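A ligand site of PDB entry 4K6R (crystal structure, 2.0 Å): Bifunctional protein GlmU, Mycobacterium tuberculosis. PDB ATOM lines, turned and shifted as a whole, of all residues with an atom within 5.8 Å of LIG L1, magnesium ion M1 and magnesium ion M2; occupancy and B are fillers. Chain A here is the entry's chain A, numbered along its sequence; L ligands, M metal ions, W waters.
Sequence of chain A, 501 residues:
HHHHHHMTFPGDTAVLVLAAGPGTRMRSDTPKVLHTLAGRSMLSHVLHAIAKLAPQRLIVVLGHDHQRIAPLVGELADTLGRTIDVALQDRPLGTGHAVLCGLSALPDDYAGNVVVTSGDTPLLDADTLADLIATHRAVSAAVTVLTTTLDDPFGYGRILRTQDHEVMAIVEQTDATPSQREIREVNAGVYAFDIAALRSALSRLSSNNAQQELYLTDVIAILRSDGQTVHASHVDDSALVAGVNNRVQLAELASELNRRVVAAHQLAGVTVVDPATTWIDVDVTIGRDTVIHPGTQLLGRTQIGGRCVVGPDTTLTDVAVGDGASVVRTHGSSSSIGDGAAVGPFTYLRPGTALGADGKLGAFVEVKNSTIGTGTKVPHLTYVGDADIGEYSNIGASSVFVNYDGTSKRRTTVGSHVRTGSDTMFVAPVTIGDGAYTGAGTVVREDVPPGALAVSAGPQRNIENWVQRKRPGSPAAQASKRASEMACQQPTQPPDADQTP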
ATOM      1  N   LEU A  18     -20.081  15.096  18.778  1.00  0.00           N
ATOM      2  CA  LEU A  18     -20.453  15.522  17.409  1.00  0.00           C
ATOM      3  C   LEU A  18     -20.375  17.020  17.354  1.00  0.00           C
ATOM      4  O   LEU A  18     -21.148  17.732  18.026  1.00  0.00           O
ATOM      5  CB  LEU A  18     -21.854  15.037  17.079  1.00  0.00           C
ATOM      6  CG  LEU A  18     -22.126  13.575  17.489  1.00  0.00           C
ATOM      7  CD1 LEU A  18     -23.543  13.143  17.088  1.00  0.00           C
ATOM      8  CD2 LEU A  18     -21.034  12.668  16.827  1.00  0.00           C
ATOM      9  N   ALA A  20     -19.740  18.786  14.020  1.00  0.00           N
ATOM     10  CA  ALA A  20     -19.428  18.930  12.589  1.00  0.00           C
ATOM     11  C   ALA A  20     -20.423  19.847  11.915  1.00  0.00           C
ATOM     12  O   ALA A  20     -20.223  20.206  10.735  1.00  0.00           O
ATOM     13  CB  ALA A  20     -19.534  17.583  11.929  1.00  0.00           C
ATOM     14  N   GLY A  21     -21.459  20.276  12.652  1.00  0.00           N
ATOM     15  CA  GLY A  21     -22.516  21.102  12.021  1.00  0.00           C
ATOM     16  C   GLY A  21     -22.068  22.522  11.722  1.00  0.00           C
ATOM     17  O   GLY A  21     -21.275  23.080  12.460  1.00  0.00           O
ATOM     18  N   PRO A  22     -22.633  23.166  10.676  1.00  0.00           N
ATOM     19  CA  PRO A  22     -22.235  24.554  10.432  1.00  0.00           C
ATOM     20  C   PRO A  22     -22.797  25.578  11.483  1.00  0.00           C
ATOM     21  O   PRO A  22     -22.314  26.715  11.536  1.00  0.00           O
ATOM     22  CB  PRO A  22     -22.887  24.908   9.074  1.00  0.00           C
ATOM     23  CG  PRO A  22     -23.350  23.601   8.501  1.00  0.00           C
ATOM     24  CD  PRO A  22     -23.637  22.677   9.715  1.00  0.00           C
ATOM     25  N   GLY A  23     -23.823  25.212  12.220  1.00  0.00           N
ATOM     26  CA  GLY A  23     -24.447  26.217  13.121  1.00  0.00           C
ATOM     27  C   GLY A  23     -24.952  27.464  12.433  1.00  0.00           C
ATOM     28  O   GLY A  23     -24.760  28.587  12.968  1.00  0.00           O
ATOM     29  N   THR A  24     -25.601  27.302  11.280  1.00  0.00           N
ATOM     30  CA  THR A  24     -26.097  28.431  10.462  1.00  0.00           C
ATOM     31  C   THR A  24     -27.064  29.307  11.279  1.00  0.00           C
ATOM     32  O   THR A  24     -27.101  30.530  11.121  1.00  0.00           O
ATOM     33  CB  THR A  24     -26.850  27.909   9.158  1.00  0.00           C
ATOM     34  OG1 THR A  24     -25.987  27.059   8.427  1.00  0.00           O
ATOM     35  CG2 THR A  24     -27.343  29.029   8.238  1.00  0.00           C
ATOM     36  N   ARG A  25     -27.851  28.667  12.140  1.00  0.00           N
ATOM     37  CA  ARG A  25     -28.788  29.405  13.053  1.00  0.00           C
ATOM     38  C   ARG A  25     -28.092  30.389  14.012  1.00  0.00           C
ATOM     39  O   ARG A  25     -28.734  31.312  14.489  1.00  0.00           O
ATOM     40  CB  ARG A  25     -29.702  28.445  13.829  1.00  0.00           C
ATOM     41  CG  ARG A  25     -30.795  27.906  12.878  1.00  0.00           C
ATOM     42  CD  ARG A  25     -31.530  26.760  13.575  1.00  0.00           C
ATOM     43  NE  ARG A  25     -30.592  25.628  13.803  1.00  0.00           N
ATOM     44  CZ  ARG A  25     -30.962  24.492  14.438  1.00  0.00           C
ATOM     45  NH1 ARG A  25     -32.190  24.391  15.000  1.00  0.00           N
ATOM     46  NH2 ARG A  25     -30.123  23.453  14.564  1.00  0.00           N
ATOM     47  N   MET A  26     -26.789  30.212  14.251  1.00  0.00           N
ATOM     48  CA  MET A  26     -25.996  31.213  15.016  1.00  0.00           C
ATOM     49  C   MET A  26     -25.782  32.496  14.250  1.00  0.00           C
ATOM     50  O   MET A  26     -25.545  33.551  14.864  1.00  0.00           O
ATOM     51  CB  MET A  26     -24.608  30.720  15.430  1.00  0.00           C
ATOM     52  CG  MET A  26     -24.638  29.393  16.202  1.00  0.00           C
ATOM     53  SD  MET A  26     -25.257  29.565  17.915  1.00  0.00           S
ATOM     54  CE  MET A  26     -23.953  30.515  18.628  1.00  0.00           C
ATOM     55  N   LYS A  32     -19.571  27.814  15.538  1.00  0.00           N
ATOM     56  CA  LYS A  32     -20.495  27.742  16.665  1.00  0.00           C
ATOM     57  C   LYS A  32     -19.924  27.164  17.932  1.00  0.00           C
ATOM     58  O   LYS A  32     -20.144  27.746  19.022  1.00  0.00           O
ATOM     59  CB  LYS A  32     -21.714  26.882  16.256  1.00  0.00           C
ATOM     60  CG  LYS A  32     -22.693  26.569  17.409  1.00  0.00           C
ATOM     61  CD  LYS A  32     -23.936  25.876  16.785  1.00  0.00           C
ATOM     62  CE  LYS A  32     -24.627  25.046  17.761  1.00  0.00           C
ATOM     63  NZ  LYS A  32     -25.693  24.157  17.084  1.00  0.00           N
ATOM     64  N   LEU A  62     -15.429  16.459  13.516  1.00  0.00           N
ATOM     65  CA  LEU A  62     -15.529  17.822  13.030  1.00  0.00           C
ATOM     66  C   LEU A  62     -15.943  17.775  11.596  1.00  0.00           C
ATOM     67  O   LEU A  62     -15.961  16.683  10.976  1.00  0.00           O
ATOM     68  CB  LEU A  62     -14.157  18.533  13.100  1.00  0.00           C
ATOM     69  CG  LEU A  62     -13.611  18.691  14.560  1.00  0.00           C
ATOM     70  CD1 LEU A  62     -12.163  19.308  14.578  1.00  0.00           C
ATOM     71  CD2 LEU A  62     -14.590  19.663  15.346  1.00  0.00           C
ATOM     72  N   GLY A  63     -16.274  18.925  11.033  1.00  0.00           N
ATOM     73  CA  GLY A  63     -16.780  18.947   9.680  1.00  0.00           C
ATOM     74  C   GLY A  63     -16.666  20.361   9.141  1.00  0.00           C
ATOM     75  O   GLY A  63     -15.590  20.828   8.760  1.00  0.00           O
ATOM     76  N   HIS A  64     -17.786  21.083   9.174  1.00  0.00           N
ATOM     77  CA  HIS A  64     -17.809  22.459   8.763  1.00  0.00           C
ATOM     78  C   HIS A  64     -16.753  23.296   9.558  1.00  0.00           C
ATOM     79  O   HIS A  64     -16.749  23.276  10.811  1.00  0.00           O
ATOM     80  CB  HIS A  64     -19.214  23.083   8.986  1.00  0.00           C
ATOM     81  CG  HIS A  64     -19.309  24.462   8.386  1.00  0.00           C
ATOM     82  ND1 HIS A  64     -19.160  25.615   9.141  1.00  0.00           N
ATOM     83  CD2 HIS A  64     -19.370  24.878   7.099  1.00  0.00           C
ATOM     84  CE1 HIS A  64     -19.256  26.684   8.348  1.00  0.00           C
ATOM     85  NE2 HIS A  64     -19.348  26.265   7.100  1.00  0.00           N
ATOM     86  N   GLN A  89     -16.185  14.641   9.208  1.00  0.00           N
ATOM     87  CA  GLN A  89     -17.391  14.347   8.505  1.00  0.00           C
ATOM     88  C   GLN A  89     -17.418  15.214   7.231  1.00  0.00           C
ATOM     89  O   GLN A  89     -17.344  16.466   7.288  1.00  0.00           O
ATOM     90  CB  GLN A  89     -18.640  14.585   9.367  1.00  0.00           C
ATOM     91  CG  GLN A  89     -19.965  14.527   8.479  1.00  0.00           C
ATOM     92  CD  GLN A  89     -21.200  14.599   9.407  1.00  0.00           C
ATOM     93  OE1 GLN A  89     -21.085  15.114  10.532  1.00  0.00           O
ATOM     94  NE2 GLN A  89     -22.359  14.021   8.990  1.00  0.00           N
ATOM     95  N   ASP A  90     -17.575  14.567   6.071  1.00  0.00           N
ATOM     96  CA  ASP A  90     -17.400  15.303   4.820  1.00  0.00           C
ATOM     97  C   ASP A  90     -18.659  15.466   3.981  1.00  0.00           C
ATOM     98  O   ASP A  90     -18.568  15.880   2.833  1.00  0.00           O
ATOM     99  CB  ASP A  90     -16.256  14.703   3.988  1.00  0.00           C
ATOM    100  CG  ASP A  90     -16.539  13.267   3.573  1.00  0.00           C
ATOM    101  OD1 ASP A  90     -15.718  12.716   2.852  1.00  0.00           O
ATOM    102  OD2 ASP A  90     -17.579  12.664   3.955  1.00  0.00           O
ATOM    103  N   ARG A  91     -19.812  15.146   4.543  1.00  0.00           N
ATOM    104  CA  ARG A  91     -21.070  15.433   3.882  1.00  0.00           C
ATOM    105  C   ARG A  91     -22.038  15.984   4.924  1.00  0.00           C
ATOM    106  O   ARG A  91     -22.007  15.504   6.086  1.00  0.00           O
ATOM    107  CB  ARG A  91     -21.659  14.116   3.380  1.00  0.00           C
ATOM    108  CG  ARG A  91     -20.935  13.545   2.169  1.00  0.00           C
ATOM    109  CD  ARG A  91     -21.755  12.322   1.710  1.00  0.00           C
ATOM    110  NE  ARG A  91     -21.452  11.083   2.463  1.00  0.00           N
ATOM    111  CZ  ARG A  91     -22.055   9.900   2.260  1.00  0.00           C
ATOM    112  NH1 ARG A  91     -23.038   9.795   1.365  1.00  0.00           N
ATOM    113  NH2 ARG A  91     -21.651   8.811   2.932  1.00  0.00           N
ATOM    114  N   PRO A  92     -22.959  16.902   4.510  1.00  0.00           N
ATOM    115  CA  PRO A  92     -23.995  17.495   5.381  1.00  0.00           C
ATOM    116  C   PRO A  92     -25.100  16.488   5.543  1.00  0.00           C
ATOM    117  O   PRO A  92     -26.220  16.709   5.133  1.00  0.00           O
ATOM    118  CB  PRO A  92     -24.514  18.719   4.577  1.00  0.00           C
ATOM    119  CG  PRO A  92     -23.446  18.965   3.546  1.00  0.00           C
ATOM    120  CD  PRO A  92     -22.860  17.612   3.227  1.00  0.00           C
ATOM    121  N   LEU A  93     -24.783  15.387   6.207  1.00  0.00           N
ATOM    122  CA  LEU A  93     -25.672  14.242   6.101  1.00  0.00           C
ATOM    123  C   LEU A  93     -26.278  13.806   7.443  1.00  0.00           C
ATOM    124  O   LEU A  93     -26.964  12.768   7.515  1.00  0.00           O
ATOM    125  CB  LEU A  93     -24.893  13.079   5.372  1.00  0.00           C
ATOM    126  CG  LEU A  93     -25.623  11.758   5.039  1.00  0.00           C
ATOM    127  CD1 LEU A  93     -26.910  11.981   4.254  1.00  0.00           C
ATOM    128  CD2 LEU A  93     -24.641  10.812   4.241  1.00  0.00           C
ATOM    129  N   GLY A  94     -26.133  14.628   8.510  1.00  0.00           N
ATOM    130  CA  GLY A  94     -26.909  14.340   9.702  1.00  0.00           C
ATOM    131  C   GLY A  94     -26.043  13.768  10.819  1.00  0.00           C
ATOM    132  O   GLY A  94     -24.895  13.264  10.639  1.00  0.00           O
ATOM    133  N   THR A  95     -26.606  13.835  12.020  1.00  0.00           N
ATOM    134  CA  THR A  95     -25.936  13.280  13.223  1.00  0.00           C
ATOM    135  C   THR A  95     -25.662  11.776  13.159  1.00  0.00           C
ATOM    136  O   THR A  95     -24.740  11.301  13.829  1.00  0.00           O
ATOM    137  CB  THR A  95     -26.765  13.548  14.471  1.00  0.00           C
ATOM    138  OG1 THR A  95     -28.122  13.110  14.232  1.00  0.00           O
ATOM    139  CG2 THR A  95     -26.769  15.149  14.737  1.00  0.00           C
ATOM    140  N   ALA A  98     -22.661  11.579  11.320  1.00  0.00           N
ATOM    141  CA  ALA A  98     -21.552  12.083  12.199  1.00  0.00           C
ATOM    142  C   ALA A  98     -21.033  10.906  13.087  1.00  0.00           C
ATOM    143  O   ALA A  98     -19.826  10.696  13.289  1.00  0.00           O
ATOM    144  CB  ALA A  98     -22.134  13.230  13.094  1.00  0.00           C
ATOM    145  N   ASP A 120     -22.686  20.938  21.393  1.00  0.00           N
ATOM    146  CA  ASP A 120     -23.475  22.172  21.755  1.00  0.00           C
ATOM    147  C   ASP A 120     -24.346  21.938  22.963  1.00  0.00           C
ATOM    148  O   ASP A 120     -25.389  22.634  23.139  1.00  0.00           O
ATOM    149  CB  ASP A 120     -24.306  22.747  20.568  1.00  0.00           C
ATOM    150  CG  ASP A 120     -25.365  21.728  19.985  1.00  0.00           C
ATOM    151  OD1 ASP A 120     -25.488  20.605  20.492  1.00  0.00           O
ATOM    152  OD2 ASP A 120     -26.146  22.057  19.066  1.00  0.00           O
ATOM    153  N   GLN A 211     -35.223  17.021   6.730  1.00  0.00           N
ATOM    154  CA  GLN A 211     -33.917  17.540   6.351  1.00  0.00           C
ATOM    155  C   GLN A 211     -33.247  16.690   5.271  1.00  0.00           C
ATOM    156  O   GLN A 211     -32.128  17.011   4.838  1.00  0.00           O
ATOM    157  CB  GLN A 211     -32.966  17.532   7.615  1.00  0.00           C
ATOM    158  CG  GLN A 211     -33.542  18.340   8.854  1.00  0.00           C
ATOM    159  CD  GLN A 211     -33.972  19.728   8.428  1.00  0.00           C
ATOM    160  OE1 GLN A 211     -33.217  20.426   7.716  1.00  0.00           O
ATOM    161  NE2 GLN A 211     -35.210  20.139   8.845  1.00  0.00           N
ATOM    162  N   GLU A 213     -31.691  13.869   5.969  1.00  0.00           N
ATOM    163  CA  GLU A 213     -30.410  13.586   6.626  1.00  0.00           C
ATOM    164  C   GLU A 213     -30.581  12.208   7.265  1.00  0.00           C
ATOM    165  O   GLU A 213     -31.728  11.726   7.419  1.00  0.00           O
ATOM    166  CB  GLU A 213     -30.188  14.605   7.758  1.00  0.00           C
ATOM    167  CG  GLU A 213     -29.650  15.963   7.241  1.00  0.00           C
ATOM    168  CD  GLU A 213     -29.653  17.036   8.331  1.00  0.00           C
ATOM    169  OE1 GLU A 213     -29.907  16.719   9.538  1.00  0.00           O
ATOM    170  OE2 GLU A 213     -29.361  18.182   7.970  1.00  0.00           O
ATOM    171  N   ASN A 245     -28.627  25.999  19.861  1.00  0.00           N
ATOM    172  CA  ASN A 245     -28.578  26.094  18.412  1.00  0.00           C
ATOM    173  C   ASN A 245     -28.592  27.495  17.872  1.00  0.00           C
ATOM    174  O   ASN A 245     -28.514  27.705  16.654  1.00  0.00           O
ATOM    175  CB  ASN A 245     -29.771  25.337  17.794  1.00  0.00           C
ATOM    176  CG  ASN A 245     -29.580  23.805  17.791  1.00  0.00           C
ATOM    177  OD1 ASN A 245     -28.455  23.273  17.893  1.00  0.00           O
ATOM    178  ND2 ASN A 245     -30.702  23.100  17.743  1.00  0.00           N
HETATM  179  P1  LIG L   1     -27.864  24.739  11.547  1.00  0.00           P
HETATM  180  O1  LIG L   1     -26.518  24.754  10.840  1.00  0.00           O
HETATM  181  O2  LIG L   1     -28.041  25.761  12.648  1.00  0.00           O
HETATM  182  O3  LIG L   1     -29.093  24.461  10.741  1.00  0.00           O
HETATM  183  P2  LIG L   1     -26.648  22.345  12.855  1.00  0.00           P
HETATM  184  O4  LIG L   1     -25.388  23.004  13.228  1.00  0.00           O
HETATM  185  O5  LIG L   1     -27.237  21.355  13.825  1.00  0.00           O
HETATM  186  O6  LIG L   1     -27.830  23.355  12.425  1.00  0.00           O
HETATM  187  P3  LIG L   1     -27.246  20.914  10.323  1.00  0.00           P
HETATM  188  O7  LIG L   1     -28.673  20.843  10.879  1.00  0.00           O
HETATM  189  O8  LIG L   1     -26.954  21.687   9.056  1.00  0.00           O
HETATM  190  O9  LIG L   1     -26.276  21.522  11.497  1.00  0.00           O
HETATM  191  O10 LIG L   1     -26.586  19.468  10.168  1.00  0.00           O
HETATM  192  C1  LIG L   1     -26.980  18.323  10.929  1.00  0.00           C
HETATM  193  C2  LIG L   1     -25.745  17.451  11.011  1.00  0.00           C
HETATM  194  O11 LIG L   1     -25.282  17.077   9.657  1.00  0.00           O
HETATM  195  C3  LIG L   1     -24.594  18.252  11.649  1.00  0.00           C
HETATM  196  O12 LIG L   1     -24.551  18.034  13.068  1.00  0.00           O
HETATM  197  C4  LIG L   1     -23.381  17.538  11.002  1.00  0.00           C
HETATM  198  O13 LIG L   1     -23.140  16.300  11.679  1.00  0.00           O
HETATM  199  C5  LIG L   1     -23.873  17.172   9.611  1.00  0.00           C
HETATM  200  N1  LIG L   1     -23.470  18.317   8.770  1.00  0.00           N
HETATM  201  C6  LIG L   1     -24.330  19.271   8.329  1.00  0.00           C
HETATM  202  N2  LIG L   1     -23.615  20.117   7.524  1.00  0.00           N
HETATM  203  C7  LIG L   1     -22.343  19.740   7.501  1.00  0.00           C
HETATM  204  C8  LIG L   1     -21.154  20.213   6.805  1.00  0.00           C
HETATM  205  N3  LIG L   1     -21.147  21.365   6.040  1.00  0.00           N
HETATM  206  N4  LIG L   1     -20.069  19.488   7.023  1.00  0.00           N
HETATM  207  C9  LIG L   1     -19.994  18.367   7.785  1.00  0.00           C
HETATM  208  N5  LIG L   1     -21.039  17.858   8.430  1.00  0.00           N
HETATM  209  C10 LIG L   1     -22.229  18.541   8.320  1.00  0.00           C
HETATM  210  C1  LG2 L   2     -30.107  17.253  18.058  1.00  0.00           C
HETATM  211  O1  LG2 L   2     -29.041  18.624  15.741  1.00  0.00           O
HETATM  212  P1  LG2 L   2     -30.099  19.429  16.458  1.00  0.00           P
HETATM  213  O2  LG2 L   2     -29.496  20.489  17.362  1.00  0.00           O
HETATM  214  O3  LG2 L   2     -31.174  19.927  15.528  1.00  0.00           O
HETATM  215  C2  LG2 L   2     -30.998  15.993  18.106  1.00  0.00           C
HETATM  216  C3  LG2 L   2     -32.283  16.319  18.883  1.00  0.00           C
HETATM  217  C4  LG2 L   2     -31.888  16.784  20.301  1.00  0.00           C
HETATM  218  C5  LG2 L   2     -30.921  17.979  20.211  1.00  0.00           C
HETATM  219  C6  LG2 L   2     -30.379  18.251  21.612  1.00  0.00           C
HETATM  220  C7  LG2 L   2     -31.394  14.337  14.620  1.00  0.00           C
HETATM  221  O4  LG2 L   2     -30.762  18.311  17.376  1.00  0.00           O
HETATM  222  O5  LG2 L   2     -33.080  15.125  18.986  1.00  0.00           O
HETATM  223  O6  LG2 L   2     -33.104  17.136  21.011  1.00  0.00           O
HETATM  224  O7  LG2 L   2     -29.782  17.668  19.375  1.00  0.00           O
HETATM  225  N1  LG2 L   2     -31.434  15.600  16.718  1.00  0.00           N
HETATM  226  C8  LG2 L   2     -30.795  14.692  15.990  1.00  0.00           C
HETATM  227  O8  LG2 L   2     -29.528  19.389  21.681  1.00  0.00           O
HETATM  228  O9  LG2 L   2     -29.748  14.200  16.362  1.00  0.00           O
HETATM  229 MG    MG M   1     -27.380  22.665   7.467  1.00  0.00          MG
HETATM  230 MG    MG M   2     -30.536  20.580  11.137  1.00  0.00          MG
HETATM  231 MG    MG M   3     -27.881  21.285  18.338  1.00  0.00          MG
HETATM  232  O   HOH W   1     -23.951  18.231  16.327  1.00  0.00           O
HETATM  233  O   HOH W   2     -25.721  21.889   6.469  1.00  0.00           O
HETATM  234  O   HOH W   3     -27.178  25.882  15.362  1.00  0.00           O
HETATM  235  O   HOH W   4     -18.786  22.976   5.156  1.00  0.00           O
HETATM  236  O   HOH W   5     -28.457  21.160   6.582  1.00  0.00           O
HETATM  237  O   HOH W   6     -26.852  21.253  16.396  1.00  0.00           O
HETATM  238  O   HOH W   7     -30.751  20.388   9.068  1.00  0.00           O
HETATM  239  O   HOH W   8     -30.544  18.618  11.267  1.00  0.00           O
HETATM  240  O   HOH W   9     -29.147  23.195   8.472  1.00  0.00           O
HETATM  241  O   HOH W  10     -24.190  22.386  15.682  1.00  0.00           O
HETATM  242  O   HOH W  11     -26.688  18.716  14.363  1.00  0.00           O
HETATM  243  O   HOH W  12     -30.944  22.665  11.027  1.00  0.00           O
HETATM  244  O   HOH W  13     -30.000  20.629  13.142  1.00  0.00           O
HETATM  245  O   HOH W  14     -22.105  17.064  14.454  1.00  0.00           O
HETATM  246  O   HOH W  15     -27.851  23.797   5.563  1.00  0.00           O
HETATM  247  O   HOH W  16     -30.463  26.324   9.396  1.00  0.00           O
HETATM  248  O   HOH W  17     -32.618  20.518  11.317  1.00  0.00           O
HETATM  249  O   HOH W  18     -26.482  24.349   8.315  1.00  0.00           O
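An oxygen (O13) of LIG L1 lies within hydrogen-bond range of the side-chain amide oxygen (OE1) of Gln 89 (2.6 Å).
O1 of LIG L1 sits at hydrogen-bond distance from N of Thr 24, at 2.7 Å.
An oxygen (O1) of LIG L1 lies within hydrogen-bond range of the side-chain hydroxyl (OG1) of Thr 24 (3.4 Å).
N of Arg 25 sits at hydrogen-bond distance from O2 of LIG L1 (3.0 Å).
NE of Arg 25 lies within salt-bridge range of O2 of LIG L1 (2.8 Å).
An oxygen (O11) of LIG L1 sits at hydrogen-bond distance from the backbone NH (N) of Gly 94 (2.8 Å).
An oxygen (O4) of LIG L1 is in hydrogen-bond range of the backbone NH (N) of Gly 23 (2.9 Å).
An oxygen (O3) of LG2 L2 lies within salt-bridge range of the guanidinium group (NH2) of Arg 25 (3.8 Å).
OG1 of Thr 95 lies within hydrogen-bond range of O9 of LG2 L2, at 2.9 Å.
The side-chain amide nitrogen (NE2) of Gln 89 is in hydrogen-bond range of the backbone carbonyl oxygen (O) of Gly 94, 3.1 Å away.
The backbone carbonyl oxygen of Arg 91 lies within hydrogen-bond range of the side-chain amide nitrogen of Gln 89 (3.3 Å).
NE2 of Gln 89 lies close to N of Ala 98, at 3.4 Å.
N of Gln 89 lies within hydrogen-bond range of O of Leu 62 (2.7 Å).
The side-chain amide nitrogen of Asn 245 lies close to the guanidinium group of Arg 25 (3.3 Å).
The backbone NH of His 64 is in hydrogen-bond range of the backbone carbonyl oxygen of Ala 20 (3.0 Å).
O of Ala 20 sits close to N5 of LIG L1 (3.4 Å).
N5 of LIG L1 sits close to O of Arg 91.
Merely in contact with LIG L1: Gly 21 (3.5 Å), Pro 22 (3.4 Å), Gly 63 (3.8 Å), His 64 (3.5 Å), Pro 92 (3.4 Å), Leu 93 (3.9 Å), Thr 95 (3.9 Å), Ala 98 (3.5 Å) and Glu 213 (3.6 Å).
No residue comes within 4 Å of magnesium ion M1.
No residue comes within 4 Å of magnesium ion M2.
Magnesium ion M1 is bound by O8 of LIG L1 (1.9 Å).
Water W5 is bound to magnesium ion M1, at 2.1 Å.
Magnesium ion M1 is bound by water W2, 2.1 Å away.
Water W18 is bound to magnesium ion M1, at 2.1 Å.
Water W9 binds magnesium ion M1, 2.1 Å away.
Water W15 is bound to magnesium ion M1, at 2.3 Å.
Magnesium ion M2 is bound by O7 of LIG L1, water W8, water W13, water W7, water W17 and water W12.
Water W7 bridges OE1 of Gln 211 and OE2 of Glu 213.
Water W11 bridges O12 of LIG L1 and O1 of LG2 L2.
Water W6 lies within hydrogen-bond range of O5 of LIG L1, NZ of Lys 32 and O1 of LG2 L2.
Water W10 bridges NZ of Lys 32 (2.7 Å) and O4 of LIG L1 (2.8 Å).
Water W3 lies within hydrogen-bond range of the backbone carbonyl oxygen (O) of Asn 245 (2.6 Å), an oxygen (O2) of LIG L1 (2.9 Å) and the side-chain amino group (NZ) of Lys 32 (2.9 Å).
Water W1 lies within hydrogen-bond range of O of Leu 18 (3.3 Å) and O12 of LIG L1 (3.3 Å).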
